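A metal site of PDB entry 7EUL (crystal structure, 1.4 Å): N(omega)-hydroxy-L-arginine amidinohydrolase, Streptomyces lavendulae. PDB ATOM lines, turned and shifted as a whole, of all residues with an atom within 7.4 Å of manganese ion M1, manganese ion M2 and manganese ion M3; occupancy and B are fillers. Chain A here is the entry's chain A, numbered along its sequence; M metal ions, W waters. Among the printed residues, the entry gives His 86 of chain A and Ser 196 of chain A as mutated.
The backbone carbonyl oxygen (O) of Ile 108 sits at hydrogen-bond distance from the backbone NH (N) of Asp 198, 2.9 Å away.
A ring nitrogen (NE2) of His 86 lies within hydrogen-bond range of the side-chain hydroxyl (OG) of Ser 196 (3.0 Å).
OE2 of Glu 241 is in hydrogen-bond range of N of His 86, 2.8 Å away.
N of Val 129 lies within hydrogen-bond range of O of Asp 113, at 3.4 Å.
A ring nitrogen (NE2) of His 86 lies close to the side-chain hydroxyl of Tyr 107 (3.4 Å).
The side-chain carboxylate of Asp 113 sits close to the side-chain hydroxyl of Tyr 107, at 2.7 Å.
The side-chain carboxylate (OD1) of Asp 200 sits close to the backbone NH (N) of Gly 110 (3.0 Å).
Of the 27 residues printed, 3 come within 4 Å of manganese ion M2.
The nearest printed residue that does not touch manganese ion M2 is Tyr 211 (4.5 Å).
Gly 110 touches manganese ion M3.
Within 4 Å of manganese ion M3: Asp 109, Gly 110, His 111, Asp 198 and Asp 200.
Manganese ion M1 is bound by the side-chain carboxylate (OD2) of Asp 109 (2.1 Å), water W1 (2.2 Å), the side-chain carboxylate (OD2) of Asp 113 (2.2 Å), water W2 (2.3 Å), a ring nitrogen (ND1) of His 86 (2.3 Å) and the side-chain carboxylate (OD2) of Asp 198 (2.3 Å).
Water W4 binds manganese ion M2 (1.9 Å).
OE1 of Glu 241 binds manganese ion M2 (2.2 Å).
OD2 of Asp 200 binds manganese ion M2 (2.3 Å).
Manganese ion M2 is bound by the side-chain carboxylate (OD2) of Asp 198 (2.4 Å).
Manganese ion M2 is bound by water W3 (2.4 Å).
The side-chain carboxylate (OD1) of Asp 198 is bound to manganese ion M2 (2.4 Å).
Manganese ion M2 has six donor atoms within binding distance.
Manganese ion M3 is bound by water W2 (1.8 Å), the side-chain carboxylate (OD2) of Asp 200 (2.0 Å), the side-chain carboxylate (OD1) of Asp 200 (2.4 Å), the side-chain carboxylate (OD1) of Asp 109 (2.5 Å) and a ring nitrogen (ND1) of His 111 (2.5 Å).
Slightly farther from manganese ion M3 lies OD2 of Asp 198 (2.9 Å).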
ATOM      1  N   MET A  18     -16.533  19.758  26.115  1.00  0.00           N
ATOM      2  CA  MET A  18     -15.859  18.628  25.499  1.00  0.00           C
ATOM      3  C   MET A  18     -15.958  17.362  26.349  1.00  0.00           C
ATOM      4  O   MET A  18     -15.992  16.268  25.776  1.00  0.00           O
ATOM      5  CB  MET A  18     -14.422  18.966  25.104  1.00  0.00           C
ATOM      6  CG  MET A  18     -14.321  19.526  23.687  1.00  0.00           C
ATOM      7  SD  MET A  18     -12.661  20.113  23.322  1.00  0.00           S
ATOM      8  CE  MET A  18     -12.382  21.005  24.862  1.00  0.00           C
ATOM      9  N   THR A  85     -10.477  15.759  25.084  1.00  0.00           N
ATOM     10  CA  THR A  85      -9.537  16.574  24.324  1.00  0.00           C
ATOM     11  C   THR A  85      -8.477  15.701  23.664  1.00  0.00           C
ATOM     12  O   THR A  85      -8.199  14.584  24.099  1.00  0.00           O
ATOM     13  CB  THR A  85      -8.815  17.606  25.204  1.00  0.00           C
ATOM     14  OG1 THR A  85      -7.966  16.932  26.145  1.00  0.00           O
ATOM     15  CG2 THR A  85      -9.808  18.490  25.956  1.00  0.00           C
ATOM     16  N   HIS A  86      -7.874  16.257  22.611  1.00  0.00           N
ATOM     17  CA  HIS A  86      -6.790  15.580  21.901  1.00  0.00           C
ATOM     18  C   HIS A  86      -5.565  15.385  22.789  1.00  0.00           C
ATOM     19  O   HIS A  86      -4.739  14.513  22.500  1.00  0.00           O
ATOM     20  CB  HIS A  86      -6.392  16.402  20.687  1.00  0.00           C
ATOM     21  CG  HIS A  86      -5.991  15.575  19.509  1.00  0.00           C
ATOM     22  ND1 HIS A  86      -5.825  16.124  18.269  1.00  0.00           N
ATOM     23  CD2 HIS A  86      -5.742  14.250  19.400  1.00  0.00           C
ATOM     24  CE1 HIS A  86      -5.528  15.153  17.404  1.00  0.00           C
ATOM     25  NE2 HIS A  86      -5.429  14.021  18.074  1.00  0.00           N
ATOM     26  N   SER A  87      -5.427  16.196  23.843  1.00  0.00           N
ATOM     27  CA  SER A  87      -4.273  16.081  24.740  1.00  0.00           C
ATOM     28  C   SER A  87      -4.218  14.734  25.463  1.00  0.00           C
ATOM     29  O   SER A  87      -3.144  14.351  25.915  1.00  0.00           O
ATOM     30  CB  SER A  87      -4.273  17.233  25.735  1.00  0.00           C
ATOM     31  OG  SER A  87      -4.065  18.484  25.064  1.00  0.00           O
ATOM     32  N   TYR A 107      -2.758  11.005  11.990  1.00  0.00           N
ATOM     33  CA  TYR A 107      -3.131  12.075  12.919  1.00  0.00           C
ATOM     34  C   TYR A 107      -4.014  13.056  12.135  1.00  0.00           C
ATOM     35  O   TYR A 107      -3.523  13.887  11.373  1.00  0.00           O
ATOM     36  CB  TYR A 107      -1.876  12.712  13.478  1.00  0.00           C
ATOM     37  CG  TYR A 107      -2.064  13.543  14.730  1.00  0.00           C
ATOM     38  CD1 TYR A 107      -2.413  14.890  14.640  1.00  0.00           C
ATOM     39  CD2 TYR A 107      -1.847  13.002  15.992  1.00  0.00           C
ATOM     40  CE1 TYR A 107      -2.585  15.672  15.797  1.00  0.00           C
ATOM     41  CE2 TYR A 107      -2.014  13.776  17.138  1.00  0.00           C
ATOM     42  CZ  TYR A 107      -2.370  15.106  17.040  1.00  0.00           C
ATOM     43  OH  TYR A 107      -2.532  15.873  18.174  1.00  0.00           O
ATOM     44  N   ILE A 108      -5.321  12.903  12.279  1.00  0.00           N
ATOM     45  CA  ILE A 108      -6.285  13.558  11.404  1.00  0.00           C
ATOM     46  C   ILE A 108      -6.780  14.784  12.143  1.00  0.00           C
ATOM     47  O   ILE A 108      -7.497  14.663  13.147  1.00  0.00           O
ATOM     48  CB  ILE A 108      -7.414  12.589  11.026  1.00  0.00           C
ATOM     49  CG1 ILE A 108      -6.817  11.286  10.450  1.00  0.00           C
ATOM     50  CG2 ILE A 108      -8.367  13.254  10.014  1.00  0.00           C
ATOM     51  CD1 ILE A 108      -7.856  10.300   9.915  1.00  0.00           C
ATOM     52  N   ASP A 109      -6.392  15.964  11.663  1.00  0.00           N
ATOM     53  CA  ASP A 109      -6.447  17.159  12.483  1.00  0.00           C
ATOM     54  C   ASP A 109      -6.386  18.382  11.583  1.00  0.00           C
ATOM     55  O   ASP A 109      -5.646  18.387  10.604  1.00  0.00           O
ATOM     56  CB  ASP A 109      -5.236  17.164  13.429  1.00  0.00           C
ATOM     57  CG  ASP A 109      -5.401  18.101  14.601  1.00  0.00           C
ATOM     58  OD1 ASP A 109      -5.423  19.323  14.422  1.00  0.00           O
ATOM     59  OD2 ASP A 109      -5.550  17.601  15.717  1.00  0.00           O
ATOM     60  N   GLY A 110      -7.121  19.435  11.940  1.00  0.00           N
ATOM     61  CA  GLY A 110      -7.042  20.670  11.183  1.00  0.00           C
ATOM     62  C   GLY A 110      -5.763  21.459  11.400  1.00  0.00           C
ATOM     63  O   GLY A 110      -5.428  22.323  10.590  1.00  0.00           O
ATOM     64  N   HIS A 111      -5.041  21.156  12.464  1.00  0.00           N
ATOM     65  CA  HIS A 111      -3.802  21.793  12.856  1.00  0.00           C
ATOM     66  C   HIS A 111      -2.687  20.736  12.833  1.00  0.00           C
ATOM     67  O   HIS A 111      -2.935  19.553  12.565  1.00  0.00           O
ATOM     68  CB  HIS A 111      -3.952  22.373  14.264  1.00  0.00           C
ATOM     69  CG  HIS A 111      -5.128  23.290  14.409  1.00  0.00           C
ATOM     70  ND1 HIS A 111      -6.353  22.860  14.861  1.00  0.00           N
ATOM     71  CD2 HIS A 111      -5.254  24.614  14.174  1.00  0.00           C
ATOM     72  CE1 HIS A 111      -7.204  23.882  14.887  1.00  0.00           C
ATOM     73  NE2 HIS A 111      -6.556  24.959  14.472  1.00  0.00           N
ATOM     74  N   GLY A 112      -1.466  21.159  13.083  1.00  0.00           N
ATOM     75  CA  GLY A 112      -0.412  20.172  13.168  1.00  0.00           C
ATOM     76  C   GLY A 112      -0.119  19.662  14.566  1.00  0.00           C
ATOM     77  O   GLY A 112       0.560  18.634  14.708  1.00  0.00           O
ATOM     78  N   ASP A 113      -0.623  20.356  15.595  1.00  0.00           N
ATOM     79  CA  ASP A 113      -0.344  20.009  16.986  1.00  0.00           C
ATOM     80  C   ASP A 113       1.143  19.718  17.219  1.00  0.00           C
ATOM     81  O   ASP A 113       1.504  18.788  17.939  1.00  0.00           O
ATOM     82  CB  ASP A 113      -1.234  18.863  17.467  1.00  0.00           C
ATOM     83  CG  ASP A 113      -2.703  19.225  17.445  1.00  0.00           C
ATOM     84  OD1 ASP A 113      -3.051  20.400  17.167  1.00  0.00           O
ATOM     85  OD2 ASP A 113      -3.514  18.332  17.736  1.00  0.00           O
ATOM     86  N   TYR A 124      -1.179  26.518  24.769  1.00  0.00           N
ATOM     87  CA  TYR A 124      -2.234  25.506  24.799  1.00  0.00           C
ATOM     88  C   TYR A 124      -1.657  24.106  24.593  1.00  0.00           C
ATOM     89  O   TYR A 124      -1.051  23.821  23.557  1.00  0.00           O
ATOM     90  CB  TYR A 124      -3.307  25.806  23.749  1.00  0.00           C
ATOM     91  CG  TYR A 124      -4.403  24.767  23.745  1.00  0.00           C
ATOM     92  CD1 TYR A 124      -4.943  24.313  24.944  1.00  0.00           C
ATOM     93  CD2 TYR A 124      -4.886  24.222  22.555  1.00  0.00           C
ATOM     94  CE1 TYR A 124      -5.931  23.352  24.967  1.00  0.00           C
ATOM     95  CE2 TYR A 124      -5.869  23.254  22.566  1.00  0.00           C
ATOM     96  CZ  TYR A 124      -6.390  22.834  23.776  1.00  0.00           C
ATOM     97  OH  TYR A 124      -7.374  21.860  23.801  1.00  0.00           O
ATOM     98  N   GLY A 126      -3.065  21.375  23.829  1.00  0.00           N
ATOM     99  CA  GLY A 126      -3.590  20.671  22.674  1.00  0.00           C
ATOM    100  C   GLY A 126      -2.838  20.945  21.385  1.00  0.00           C
ATOM    101  O   GLY A 126      -2.939  20.161  20.435  1.00  0.00           O
ATOM    102  N   GLY A 127      -2.097  22.045  21.332  1.00  0.00           N
ATOM    103  CA  GLY A 127      -1.256  22.339  20.191  1.00  0.00           C
ATOM    104  C   GLY A 127       0.126  21.751  20.248  1.00  0.00           C
ATOM    105  O   GLY A 127       0.949  22.062  19.375  1.00  0.00           O
ATOM    106  N   VAL A 129       0.596  18.173  21.113  1.00  0.00           N
ATOM    107  CA  VAL A 129       0.383  16.744  21.345  1.00  0.00           C
ATOM    108  C   VAL A 129       1.309  15.879  20.492  1.00  0.00           C
ATOM    109  O   VAL A 129       1.950  14.953  20.999  1.00  0.00           O
ATOM    110  CB  VAL A 129      -1.095  16.403  21.091  1.00  0.00           C
ATOM    111  CG1 VAL A 129      -1.320  14.926  21.243  1.00  0.00           C
ATOM    112  CG2 VAL A 129      -2.007  17.185  22.023  1.00  0.00           C
ATOM    113  N   SER A 196      -6.011   8.746  14.958  1.00  0.00           N
ATOM    114  CA  SER A 196      -6.339   9.728  15.999  1.00  0.00           C
ATOM    115  C   SER A 196      -6.981  10.928  15.335  1.00  0.00           C
ATOM    116  O   SER A 196      -6.321  11.620  14.546  1.00  0.00           O
ATOM    117  CB  SER A 196      -5.075  10.160  16.735  1.00  0.00           C
ATOM    118  OG  SER A 196      -5.380  11.048  17.803  1.00  0.00           O
ATOM    119  N   ILE A 197      -8.254  11.200  15.640  1.00  0.00           N
ATOM    120  CA  ILE A 197      -9.050  12.204  14.957  1.00  0.00           C
ATOM    121  C   ILE A 197      -9.414  13.339  15.935  1.00  0.00           C
ATOM    122  O   ILE A 197      -9.866  13.055  17.046  1.00  0.00           O
ATOM    123  CB  ILE A 197     -10.351  11.608  14.396  1.00  0.00           C
ATOM    124  CG1 ILE A 197     -10.053  10.639  13.263  1.00  0.00           C
ATOM    125  CG2 ILE A 197     -11.296  12.717  13.924  1.00  0.00           C
ATOM    126  CD1 ILE A 197     -11.260   9.856  12.811  1.00  0.00           C
ATOM    127  N   ASP A 198      -9.250  14.581  15.485  1.00  0.00           N
ATOM    128  CA  ASP A 198      -9.738  15.795  16.155  1.00  0.00           C
ATOM    129  C   ASP A 198     -10.785  16.365  15.204  1.00  0.00           C
ATOM    130  O   ASP A 198     -10.461  16.651  14.041  1.00  0.00           O
ATOM    131  CB  ASP A 198      -8.550  16.752  16.296  1.00  0.00           C
ATOM    132  CG  ASP A 198      -8.876  18.074  16.967  1.00  0.00           C
ATOM    133  OD1 ASP A 198     -10.013  18.575  16.868  1.00  0.00           O
ATOM    134  OD2 ASP A 198      -7.971  18.655  17.595  1.00  0.00           O
ATOM    135  N   TRP A 199     -12.029  16.515  15.673  1.00  0.00           N
ATOM    136  CA  TRP A 199     -13.117  16.951  14.778  1.00  0.00           C
ATOM    137  C   TRP A 199     -12.927  18.344  14.184  1.00  0.00           C
ATOM    138  O   TRP A 199     -13.659  18.688  13.250  1.00  0.00           O
ATOM    139  CB  TRP A 199     -14.501  16.826  15.428  1.00  0.00           C
ATOM    140  CG  TRP A 199     -14.822  15.423  15.860  1.00  0.00           C
ATOM    141  CD1 TRP A 199     -15.121  15.015  17.124  1.00  0.00           C
ATOM    142  CD2 TRP A 199     -14.854  14.238  15.035  1.00  0.00           C
ATOM    143  NE1 TRP A 199     -15.344  13.656  17.145  1.00  0.00           N
ATOM    144  CE2 TRP A 199     -15.182  13.161  15.883  1.00  0.00           C
ATOM    145  CE3 TRP A 199     -14.636  14.000  13.678  1.00  0.00           C
ATOM    146  CZ2 TRP A 199     -15.310  11.853  15.415  1.00  0.00           C
ATOM    147  CZ3 TRP A 199     -14.750  12.687  13.209  1.00  0.00           C
ATOM    148  CH2 TRP A 199     -15.084  11.633  14.084  1.00  0.00           C
ATOM    149  N   ASP A 200     -11.952  19.142  14.650  1.00  0.00           N
ATOM    150  CA  ASP A 200     -11.673  20.390  13.937  1.00  0.00           C
ATOM    151  C   ASP A 200     -11.063  20.170  12.553  1.00  0.00           C
ATOM    152  O   ASP A 200     -10.861  21.143  11.806  1.00  0.00           O
ATOM    153  CB  ASP A 200     -10.849  21.376  14.790  1.00  0.00           C
ATOM    154  CG  ASP A 200      -9.415  20.910  15.074  1.00  0.00           C
ATOM    155  OD1 ASP A 200      -8.813  20.187  14.256  1.00  0.00           O
ATOM    156  OD2 ASP A 200      -8.883  21.307  16.132  1.00  0.00           O
ATOM    157  N   VAL A 201     -10.768  18.915  12.174  1.00  0.00           N
ATOM    158  CA  VAL A 201     -10.335  18.629  10.809  1.00  0.00           C
ATOM    159  C   VAL A 201     -11.449  18.909   9.801  1.00  0.00           C
ATOM    160  O   VAL A 201     -11.179  19.191   8.638  1.00  0.00           O
ATOM    161  CB  VAL A 201      -9.801  17.193  10.700  1.00  0.00           C
ATOM    162  CG1 VAL A 201     -10.957  16.169  10.752  1.00  0.00           C
ATOM    163  CG2 VAL A 201      -8.985  17.040   9.435  1.00  0.00           C
ATOM    164  N   ALA A 209     -16.483  21.753  17.333  1.00  0.00           N
ATOM    165  CA  ALA A 209     -15.254  21.416  18.039  1.00  0.00           C
ATOM    166  C   ALA A 209     -14.774  22.638  18.813  1.00  0.00           C
ATOM    167  O   ALA A 209     -15.579  23.495  19.183  1.00  0.00           O
ATOM    168  CB  ALA A 209     -14.187  20.890  17.061  1.00  0.00           C
ATOM    169  N   ASP A 210     -13.475  22.723  19.087  1.00  0.00           N
ATOM    170  CA  ASP A 210     -12.957  23.888  19.788  1.00  0.00           C
ATOM    171  C   ASP A 210     -12.501  24.966  18.812  1.00  0.00           C
ATOM    172  O   ASP A 210     -12.751  26.157  19.037  1.00  0.00           O
ATOM    173  CB  ASP A 210     -11.795  23.471  20.709  1.00  0.00           C
ATOM    174  CG  ASP A 210     -11.441  24.539  21.741  1.00  0.00           C
ATOM    175  OD1 ASP A 210     -12.086  25.599  21.762  1.00  0.00           O
ATOM    176  OD2 ASP A 210     -10.508  24.284  22.535  1.00  0.00           O
ATOM    177  N   TYR A 211     -11.861  24.565  17.722  1.00  0.00           N
ATOM    178  CA  TYR A 211     -11.352  25.487  16.737  1.00  0.00           C
ATOM    179  C   TYR A 211     -12.090  25.323  15.423  1.00  0.00           C
ATOM    180  O   TYR A 211     -12.682  24.279  15.122  1.00  0.00           O
ATOM    181  CB  TYR A 211      -9.845  25.300  16.541  1.00  0.00           C
ATOM    182  CG  TYR A 211      -9.067  25.739  17.759  1.00  0.00           C
ATOM    183  CD1 TYR A 211      -8.962  24.902  18.870  1.00  0.00           C
ATOM    184  CD2 TYR A 211      -8.485  26.997  17.823  1.00  0.00           C
ATOM    185  CE1 TYR A 211      -8.270  25.298  20.002  1.00  0.00           C
ATOM    186  CE2 TYR A 211      -7.792  27.399  18.942  1.00  0.00           C
ATOM    187  CZ  TYR A 211      -7.690  26.552  20.032  1.00  0.00           C
ATOM    188  OH  TYR A 211      -6.997  26.955  21.151  1.00  0.00           O
ATOM    189  N   VAL A 213     -11.307  25.930  11.595  1.00  0.00           N
ATOM    190  CA  VAL A 213     -10.366  26.158  10.511  1.00  0.00           C
ATOM    191  C   VAL A 213     -11.129  26.032   9.189  1.00  0.00           C
ATOM    192  O   VAL A 213     -11.685  24.955   8.924  1.00  0.00           O
ATOM    193  CB  VAL A 213      -9.205  25.162  10.564  1.00  0.00           C
ATOM    194  CG1 VAL A 213      -8.031  25.693   9.783  1.00  0.00           C
ATOM    195  CG2 VAL A 213      -8.811  24.885  12.017  1.00  0.00           C
ATOM    196  N   ALA A 240     -11.808  12.636  19.274  1.00  0.00           N
ATOM    197  CA  ALA A 240     -11.638  13.721  20.239  1.00  0.00           C
ATOM    198  C   ALA A 240     -12.262  15.017  19.760  1.00  0.00           C
ATOM    199  O   ALA A 240     -12.266  15.329  18.565  1.00  0.00           O
ATOM    200  CB  ALA A 240     -10.144  13.994  20.500  1.00  0.00           C
ATOM    201  N   GLU A 241     -12.769  15.777  20.734  1.00  0.00           N
ATOM    202  CA  GLU A 241     -13.105  17.191  20.624  1.00  0.00           C
ATOM    203  C   GLU A 241     -14.467  17.495  20.021  1.00  0.00           C
ATOM    204  O   GLU A 241     -14.619  18.435  19.235  1.00  0.00           O
ATOM    205  CB  GLU A 241     -11.988  17.990  19.955  1.00  0.00           C
ATOM    206  CG  GLU A 241     -10.612  17.648  20.509  1.00  0.00           C
ATOM    207  CD  GLU A 241      -9.794  18.856  20.844  1.00  0.00           C
ATOM    208  OE1 GLU A 241     -10.025  19.914  20.243  1.00  0.00           O
ATOM    209  OE2 GLU A 241      -8.894  18.739  21.711  1.00  0.00           O
HETATM  210 MN    MN M   1      -5.710  18.312  17.705  1.00  0.00          MN
HETATM  211 MN    MN M   2      -9.399  20.436  18.245  1.00  0.00          MN
HETATM  212 MN    MN M   3      -7.001  20.652  15.744  1.00  0.00          MN
HETATM  213  O   HOH W   1      -5.466  19.186  19.701  1.00  0.00           O
HETATM  214  O   HOH W   2      -5.752  20.450  17.004  1.00  0.00           O
HETATM  215  O   HOH W   3      -7.484  21.576  19.073  1.00  0.00           O
HETATM  216  O   HOH W   4     -10.785  21.729  18.316  1.00  0.00           O
